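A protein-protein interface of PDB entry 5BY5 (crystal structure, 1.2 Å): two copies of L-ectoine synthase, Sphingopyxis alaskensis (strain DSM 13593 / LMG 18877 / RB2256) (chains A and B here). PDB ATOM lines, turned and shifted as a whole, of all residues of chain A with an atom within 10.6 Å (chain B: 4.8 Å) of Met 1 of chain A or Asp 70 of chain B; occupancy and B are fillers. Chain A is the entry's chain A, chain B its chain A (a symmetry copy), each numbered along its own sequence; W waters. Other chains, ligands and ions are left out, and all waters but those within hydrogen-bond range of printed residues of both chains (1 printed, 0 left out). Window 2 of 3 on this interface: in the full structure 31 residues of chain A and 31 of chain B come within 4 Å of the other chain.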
ATOM      1  N   MET A   1       9.631 -26.858 -24.714  1.00  0.00           N
ATOM      2  CA  MET A   1       8.818 -27.656 -23.763  1.00  0.00           C
ATOM      3  C   MET A   1       8.010 -26.695 -22.929  1.00  0.00           C
ATOM      4  O   MET A   1       8.502 -25.621 -22.572  1.00  0.00           O
ATOM      5  CB  MET A   1       9.801 -28.456 -22.820  1.00  0.00           C
ATOM      6  CG  MET A   1       9.304 -29.256 -21.691  1.00  0.00           C
ATOM      7  SD  MET A   1      10.694 -29.674 -20.606  1.00  0.00           S
ATOM      8  CE  MET A   1      11.703 -30.635 -21.686  1.00  0.00           C
ATOM      9  N   ILE A   2       6.785 -27.073 -22.565  1.00  0.00           N
ATOM     10  CA  ILE A   2       5.988 -26.420 -21.527  1.00  0.00           C
ATOM     11  C   ILE A   2       6.048 -27.265 -20.270  1.00  0.00           C
ATOM     12  O   ILE A   2       5.933 -28.500 -20.347  1.00  0.00           O
ATOM     13  CB  ILE A   2       4.521 -26.303 -21.992  1.00  0.00           C
ATOM     14  CG1 ILE A   2       4.385 -25.285 -23.120  1.00  0.00           C
ATOM     15  CG2 ILE A   2       3.641 -25.966 -20.822  1.00  0.00           C
ATOM     16  CD1 ILE A   2       3.024 -25.327 -23.782  1.00  0.00           C
ATOM     17  N   VAL A   3       6.225 -26.617 -19.120  1.00  0.00           N
ATOM     18  CA  VAL A   3       6.080 -27.276 -17.824  1.00  0.00           C
ATOM     19  C   VAL A   3       5.329 -26.370 -16.911  1.00  0.00           C
ATOM     20  O   VAL A   3       5.756 -25.223 -16.705  1.00  0.00           O
ATOM     21  CB  VAL A   3       7.419 -27.673 -17.175  1.00  0.00           C
ATOM     22  CG1 VAL A   3       7.108 -28.481 -15.905  1.00  0.00           C
ATOM     23  CG2 VAL A   3       8.334 -28.411 -18.106  1.00  0.00           C
ATOM     24  N   ARG A   4       4.174 -26.778 -16.387  1.00  0.00           N
ATOM     25  CA  ARG A   4       3.291 -25.926 -15.582  1.00  0.00           C
ATOM     26  C   ARG A   4       2.684 -26.746 -14.487  1.00  0.00           C
ATOM     27  O   ARG A   4       2.577 -27.948 -14.576  1.00  0.00           O
ATOM     28  CB  ARG A   4       2.121 -25.408 -16.391  1.00  0.00           C
ATOM     29  CG  ARG A   4       2.501 -24.622 -17.498  1.00  0.00           C
ATOM     30  CD  ARG A   4       1.264 -24.253 -18.330  1.00  0.00           C
ATOM     31  NE  ARG A   4       1.902 -23.439 -19.276  1.00  0.00           N
ATOM     32  CZ  ARG A   4       1.450 -23.120 -20.460  1.00  0.00           C
ATOM     33  NH1 ARG A   4       0.270 -23.551 -20.910  1.00  0.00           N
ATOM     34  NH2 ARG A   4       2.228 -22.366 -21.217  1.00  0.00           N
ATOM     35  N   LEU A  27      -3.776 -26.394 -20.794  1.00  0.00           N
ATOM     36  CA  LEU A  27      -3.558 -26.126 -22.202  1.00  0.00           C
ATOM     37  C   LEU A  27      -4.876 -25.670 -22.810  1.00  0.00           C
ATOM     38  O   LEU A  27      -5.911 -26.321 -22.574  1.00  0.00           O
ATOM     39  CB  LEU A  27      -3.036 -27.357 -22.948  1.00  0.00           C
ATOM     40  CG  LEU A  27      -1.684 -27.871 -22.506  1.00  0.00           C
ATOM     41  CD1 LEU A  27      -1.446 -29.255 -23.090  1.00  0.00           C
ATOM     42  CD2 LEU A  27      -0.581 -26.929 -22.874  1.00  0.00           C
ATOM     43  N   ASP A  31      -2.034 -22.450 -26.762  1.00  0.00           N
ATOM     44  CA  ASP A  31      -0.846 -23.232 -26.494  1.00  0.00           C
ATOM     45  C   ASP A  31      -0.404 -24.082 -27.661  1.00  0.00           C
ATOM     46  O   ASP A  31       0.693 -24.650 -27.613  1.00  0.00           O
ATOM     47  CB  ASP A  31      -1.035 -24.103 -25.257  1.00  0.00           C
ATOM     48  CG  ASP A  31      -1.243 -23.291 -23.990  1.00  0.00           C
ATOM     49  OD1 ASP A  31      -0.308 -22.604 -23.557  1.00  0.00           O
ATOM     50  OD2 ASP A  31      -2.333 -23.352 -23.425  1.00  0.00           O
ATOM     51  N   MET A  33      -1.218 -27.018 -29.130  1.00  0.00           N
ATOM     52  CA  MET A  33      -1.120 -28.463 -29.157  1.00  0.00           C
ATOM     53  C   MET A  33      -2.175 -29.154 -29.992  1.00  0.00           C
ATOM     54  O   MET A  33      -2.087 -30.370 -30.222  1.00  0.00           O
ATOM     55  CB  MET A  33      -1.129 -29.023 -27.744  1.00  0.00           C
ATOM     56  CG  MET A  33       0.061 -28.568 -26.879  1.00  0.00           C
ATOM     57  SD  MET A  33       1.619 -29.351 -27.299  1.00  0.00           S
ATOM     58  CE  MET A  33       1.321 -30.969 -26.631  1.00  0.00           C
ATOM     59  N   ILE B  68      12.074 -33.762 -14.749  1.00  0.00           N
ATOM     60  CA  ILE B  68      12.231 -33.696 -16.201  1.00  0.00           C
ATOM     61  C   ILE B  68      13.251 -32.595 -16.497  1.00  0.00           C
ATOM     62  O   ILE B  68      13.097 -31.456 -16.045  1.00  0.00           O
ATOM     63  CB  ILE B  68      10.909 -33.487 -16.997  1.00  0.00           C
ATOM     64  CG1 ILE B  68      11.192 -33.492 -18.503  1.00  0.00           C
ATOM     65  CG2 ILE B  68      10.136 -32.248 -16.584  1.00  0.00           C
ATOM     66  CD1 ILE B  68       9.941 -33.525 -19.359  1.00  0.00           C
ATOM     67  N   GLU B  69      14.299 -32.962 -17.213  1.00  0.00           N
ATOM     68  CA  GLU B  69      15.375 -32.049 -17.558  1.00  0.00           C
ATOM     69  C   GLU B  69      15.263 -31.685 -19.016  1.00  0.00           C
ATOM     70  O   GLU B  69      15.072 -32.548 -19.880  1.00  0.00           O
ATOM     71  CB  GLU B  69      16.714 -32.690 -17.260  1.00  0.00           C
ATOM     72  CG  GLU B  69      17.888 -31.765 -17.468  1.00  0.00           C
ATOM     73  CD  GLU B  69      19.177 -32.190 -16.808  1.00  0.00           C
ATOM     74  OE1 GLU B  69      19.337 -33.321 -16.307  1.00  0.00           O
ATOM     75  OE2 GLU B  69      20.085 -31.330 -16.695  1.00  0.00           O
ATOM     76  N   ASP B  70      15.326 -30.389 -19.283  1.00  0.00           N
ATOM     77  CA  ASP B  70      15.303 -29.860 -20.624  1.00  0.00           C
ATOM     78  C   ASP B  70      16.724 -29.604 -21.094  1.00  0.00           C
ATOM     79  O   ASP B  70      17.395 -28.712 -20.592  1.00  0.00           O
ATOM     80  CB  ASP B  70      14.511 -28.549 -20.622  1.00  0.00           C
ATOM     81  CG  ASP B  70      14.295 -27.962 -21.986  1.00  0.00           C
ATOM     82  OD1 ASP B  70      14.994 -28.304 -22.956  1.00  0.00           O
ATOM     83  OD2 ASP B  70      13.381 -27.108 -22.084  1.00  0.00           O
ATOM     84  N   LEU B  71      17.194 -30.430 -22.011  1.00  0.00           N
ATOM     85  CA  LEU B  71      18.579 -30.328 -22.470  1.00  0.00           C
ATOM     86  C   LEU B  71      18.821 -29.086 -23.333  1.00  0.00           C
ATOM     87  O   LEU B  71      19.965 -28.678 -23.508  1.00  0.00           O
ATOM     88  CB  LEU B  71      18.988 -31.600 -23.231  1.00  0.00           C
ATOM     89  CG  LEU B  71      18.815 -32.942 -22.498  1.00  0.00           C
ATOM     90  CD1 LEU B  71      19.171 -34.128 -23.350  1.00  0.00           C
ATOM     91  CD2 LEU B  71      19.498 -32.948 -21.150  1.00  0.00           C
ATOM     92  N   ALA B  72      17.800 -28.435 -23.825  1.00  0.00           N
ATOM     93  CA  ALA B  72      17.981 -27.186 -24.580  1.00  0.00           C
ATOM     94  C   ALA B  72      18.342 -26.021 -23.668  1.00  0.00           C
ATOM     95  O   ALA B  72      19.011 -25.077 -24.107  1.00  0.00           O
ATOM     96  CB  ALA B  72      16.716 -26.837 -25.392  1.00  0.00           C
ATOM     97  N   THR B  73      17.949 -26.067 -22.410  1.00  0.00           N
ATOM     98  CA  THR B  73      18.152 -24.971 -21.489  1.00  0.00           C
ATOM     99  C   THR B  73      18.893 -25.287 -20.207  1.00  0.00           C
ATOM    100  O   THR B  73      19.381 -24.394 -19.536  1.00  0.00           O
ATOM    101  CB  THR B  73      16.831 -24.360 -21.093  1.00  0.00           C
ATOM    102  OG1 THR B  73      16.145 -25.356 -20.338  1.00  0.00           O
ATOM    103  CG2 THR B  73      16.046 -23.929 -22.319  1.00  0.00           C
ATOM    104  N   GLY B  74      19.011 -26.550 -19.893  1.00  0.00           N
ATOM    105  CA  GLY B  74      19.550 -26.989 -18.595  1.00  0.00           C
ATOM    106  C   GLY B  74      18.589 -26.856 -17.436  1.00  0.00           C
ATOM    107  O   GLY B  74      18.982 -27.072 -16.287  1.00  0.00           O
ATOM    108  N   GLU B  75      17.349 -26.546 -17.701  1.00  0.00           N
ATOM    109  CA  GLU B  75      16.392 -26.464 -16.640  1.00  0.00           C
ATOM    110  C   GLU B  75      16.013 -27.863 -16.164  1.00  0.00           C
ATOM    111  O   GLU B  75      15.678 -28.731 -16.959  1.00  0.00           O
ATOM    112  CB  GLU B  75      15.124 -25.731 -17.105  1.00  0.00           C
ATOM    113  CG  GLU B  75      15.292 -24.247 -17.364  1.00  0.00           C
ATOM    114  CD  GLU B  75      14.191 -23.629 -18.172  1.00  0.00           C
ATOM    115  OE1 GLU B  75      13.989 -24.018 -19.333  1.00  0.00           O
ATOM    116  OE2 GLU B  75      13.560 -22.676 -17.697  1.00  0.00           O
ATOM    117  N   HIS B  77      13.185 -29.568 -13.953  1.00  0.00           N
ATOM    118  CA  HIS B  77      11.866 -29.299 -13.411  1.00  0.00           C
ATOM    119  C   HIS B  77      11.441 -30.443 -12.485  1.00  0.00           C
ATOM    120  O   HIS B  77      11.608 -31.604 -12.794  1.00  0.00           O
ATOM    121  CB  HIS B  77      10.829 -29.240 -14.535  1.00  0.00           C
ATOM    122  CG  HIS B  77      11.108 -28.258 -15.606  1.00  0.00           C
ATOM    123  ND1 HIS B  77      10.614 -26.986 -15.594  1.00  0.00           N
ATOM    124  CD2 HIS B  77      11.821 -28.358 -16.759  1.00  0.00           C
ATOM    125  CE1 HIS B  77      10.973 -26.332 -16.684  1.00  0.00           C
ATOM    126  NE2 HIS B  77      11.707 -27.144 -17.421  1.00  0.00           N
ATOM    127  N   ALA B  86       4.550 -30.621 -21.694  1.00  0.00           N
ATOM    128  CA  ALA B  86       4.156 -30.806 -23.069  1.00  0.00           C
ATOM    129  C   ALA B  86       5.406 -30.740 -23.945  1.00  0.00           C
ATOM    130  O   ALA B  86       6.264 -29.872 -23.749  1.00  0.00           O
ATOM    131  CB  ALA B  86       3.122 -29.811 -23.535  1.00  0.00           C
ATOM    132  N   LEU B  87       5.464 -31.665 -24.899  1.00  0.00           N
ATOM    133  CA  LEU B  87       6.631 -31.927 -25.714  1.00  0.00           C
ATOM    134  C   LEU B  87       6.274 -31.984 -27.199  1.00  0.00           C
ATOM    135  O   LEU B  87       5.202 -32.436 -27.588  1.00  0.00           O
ATOM    136  CB  LEU B  87       7.252 -33.299 -25.351  1.00  0.00           C
ATOM    137  CG  LEU B  87       7.676 -33.495 -23.898  1.00  0.00           C
ATOM    138  CD1 LEU B  87       8.021 -34.950 -23.655  1.00  0.00           C
ATOM    139  CD2 LEU B  87       8.819 -32.581 -23.524  1.00  0.00           C
ATOM    140  N   ASP B  91      11.943 -31.025 -28.828  1.00  0.00           N
ATOM    141  CA  ASP B  91      12.388 -31.053 -27.438  1.00  0.00           C
ATOM    142  C   ASP B  91      13.417 -32.110 -27.215  1.00  0.00           C
ATOM    143  O   ASP B  91      13.448 -33.130 -27.932  1.00  0.00           O
ATOM    144  CB  ASP B  91      11.196 -31.219 -26.475  1.00  0.00           C
ATOM    145  CG  ASP B  91      10.363 -29.970 -26.348  1.00  0.00           C
ATOM    146  OD1 ASP B  91      10.982 -28.883 -26.124  1.00  0.00           O
ATOM    147  OD2 ASP B  91       9.128 -30.036 -26.437  1.00  0.00           O
ATOM    148  N   ARG B  92      14.342 -31.833 -26.355  1.00  0.00           N
ATOM    149  CA  ARG B  92      15.371 -32.759 -25.938  1.00  0.00           C
ATOM    150  C   ARG B  92      15.254 -32.853 -24.454  1.00  0.00           C
ATOM    151  O   ARG B  92      15.427 -31.861 -23.786  1.00  0.00           O
ATOM    152  CB  ARG B  92      16.737 -32.242 -26.353  1.00  0.00           C
ATOM    153  CG  ARG B  92      16.893 -32.102 -27.867  1.00  0.00           C
ATOM    154  CD  ARG B  92      18.183 -31.329 -28.298  1.00  0.00           C
ATOM    155  NE  ARG B  92      19.380 -31.861 -27.655  1.00  0.00           N
ATOM    156  CZ  ARG B  92      20.312 -31.152 -26.998  1.00  0.00           C
ATOM    157  NH1 ARG B  92      20.201 -29.811 -26.835  1.00  0.00           N
ATOM    158  NH2 ARG B  92      21.344 -31.797 -26.470  1.00  0.00           N
ATOM    159  N   HIS B  93      14.795 -33.975 -23.936  1.00  0.00           N
ATOM    160  CA  HIS B  93      14.367 -34.109 -22.545  1.00  0.00           C
ATOM    161  C   HIS B  93      14.783 -35.428 -21.994  1.00  0.00           C
ATOM    162  O   HIS B  93      14.953 -36.401 -22.718  1.00  0.00           O
ATOM    163  CB  HIS B  93      12.821 -33.954 -22.447  1.00  0.00           C
ATOM    164  CG  HIS B  93      12.098 -35.066 -23.075  1.00  0.00           C
ATOM    165  ND1 HIS B  93      11.938 -35.133 -24.425  1.00  0.00           N
ATOM    166  CD2 HIS B  93      11.607 -36.209 -22.561  1.00  0.00           C
ATOM    167  CE1 HIS B  93      11.358 -36.272 -24.733  1.00  0.00           C
ATOM    168  NE2 HIS B  93      11.152 -36.948 -23.614  1.00  0.00           N
HETATM  169  O   HOH W   1       7.803 -27.848 -27.091  1.00  0.00           O
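The backbone NH of Asp 70 of chain B is in hydrogen-bond range of the backbone carbonyl oxygen of Glu 75 of chain B (2.9 Å).
The side-chain carboxylate (OD1) of Asp 70 of chain B sits at hydrogen-bond distance from the backbone NH (N) of Ala 72 of chain B (2.9 Å).
The backbone NH of His 77 of chain B is in hydrogen-bond range of the backbone carbonyl oxygen of Ile 68 of chain B (2.8 Å).
No position is printed for both chains.
Of the 8 pairs that touch across the chains among the printed residues, none has its exchanged pair printed and touching as well.
Met 1 of chain A touches Asp 70 of chain B.
O of Ala 86 of chain B touches CA of Met 1 of chain A (3.4 Å).
Met 1 of chain A touches Leu 87 of chain B.
Met 1 of chain A touches His 93 of chain B.
His 77 of chain B touches Val 3 of chain A (ND1 to CB, 3.6 Å).
CE of Met 33 of chain A touches CB of Ala 86 of chain B, at 3.8 Å.
The backbone NH of Ala 86 of chain B lies within hydrogen-bond range of the backbone carbonyl oxygen of Ile 2 of chain A (2.9 Å).
OD1 of Asp 91 of chain B is in hydrogen-bond range of N of Met 1 of chain A, at 2.8 Å.
Water W1 lies within hydrogen-bond range of OD2 of Asp 91 of chain B (2.6 Å) and N of Met 1 of chain A (3.2 Å).
Of the 7 printed residues of chain A, 4 touch a printed residue of chain B.
Hydrophobic or aromatic side chains of chain A within 4 Å of the printed part of chain B: Met 1, Val 3 and Met 33.
Along chain A the printed residues that touch a printed residue of chain B span positions 1 to 33.
Of the 14 printed residues of chain B, 6 touch a printed residue of chain A.
Printed residues of chain B that touch a printed residue of chain A: Asp 70, His 77, Ala 86, Leu 87, Asp 91 and His 93.
Hydrophobic or aromatic side chains of chain B within 4 Å of the printed part of chain A: His 77, Ala 86, Leu 87 and His 93.
Along chain B the printed residues that touch a printed residue of chain A span positions 70 to 93.
Of the printed residues of chain B, Met 1 of chain A touches Asp 70, Ala 86, Leu 87, Asp 91 and His 93.
Printed residues of chain B within 4 Å of Ile 2 of chain A: Ala 86 (2.9 Å).
Asp 31 of chain A touches none of the printed residues of chain B.
Of the printed residues of chain B, Met 33 of chain A touches Ala 86.
No residue of chain A comes within 4 Å of Ile 68 of chain B.
No residue of chain A comes within 4 Å of Glu 69 of chain B.
Asp 70 of chain B touches just one residue of chain A: Met 1 (3.7 Å).
No residue of chain A comes within 4 Å of Leu 71 of chain B.
No residue of chain A comes within 4 Å of Glu 75 of chain B.
Of the printed residues of chain A, His 77 of chain B touches Val 3.
Of chain A, only Met 1 (3.4 Å), Ile 2 (2.9 Å) and Met 33 (3.8 Å) come within 4 Å of Ala 86 of chain B.
Arg 92 of chain B touches none of the printed residues of chain A.
The nearest printed residue of chain B that does not touch Val 3 of chain A is Ile 68 of chain B (4.5 Å).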
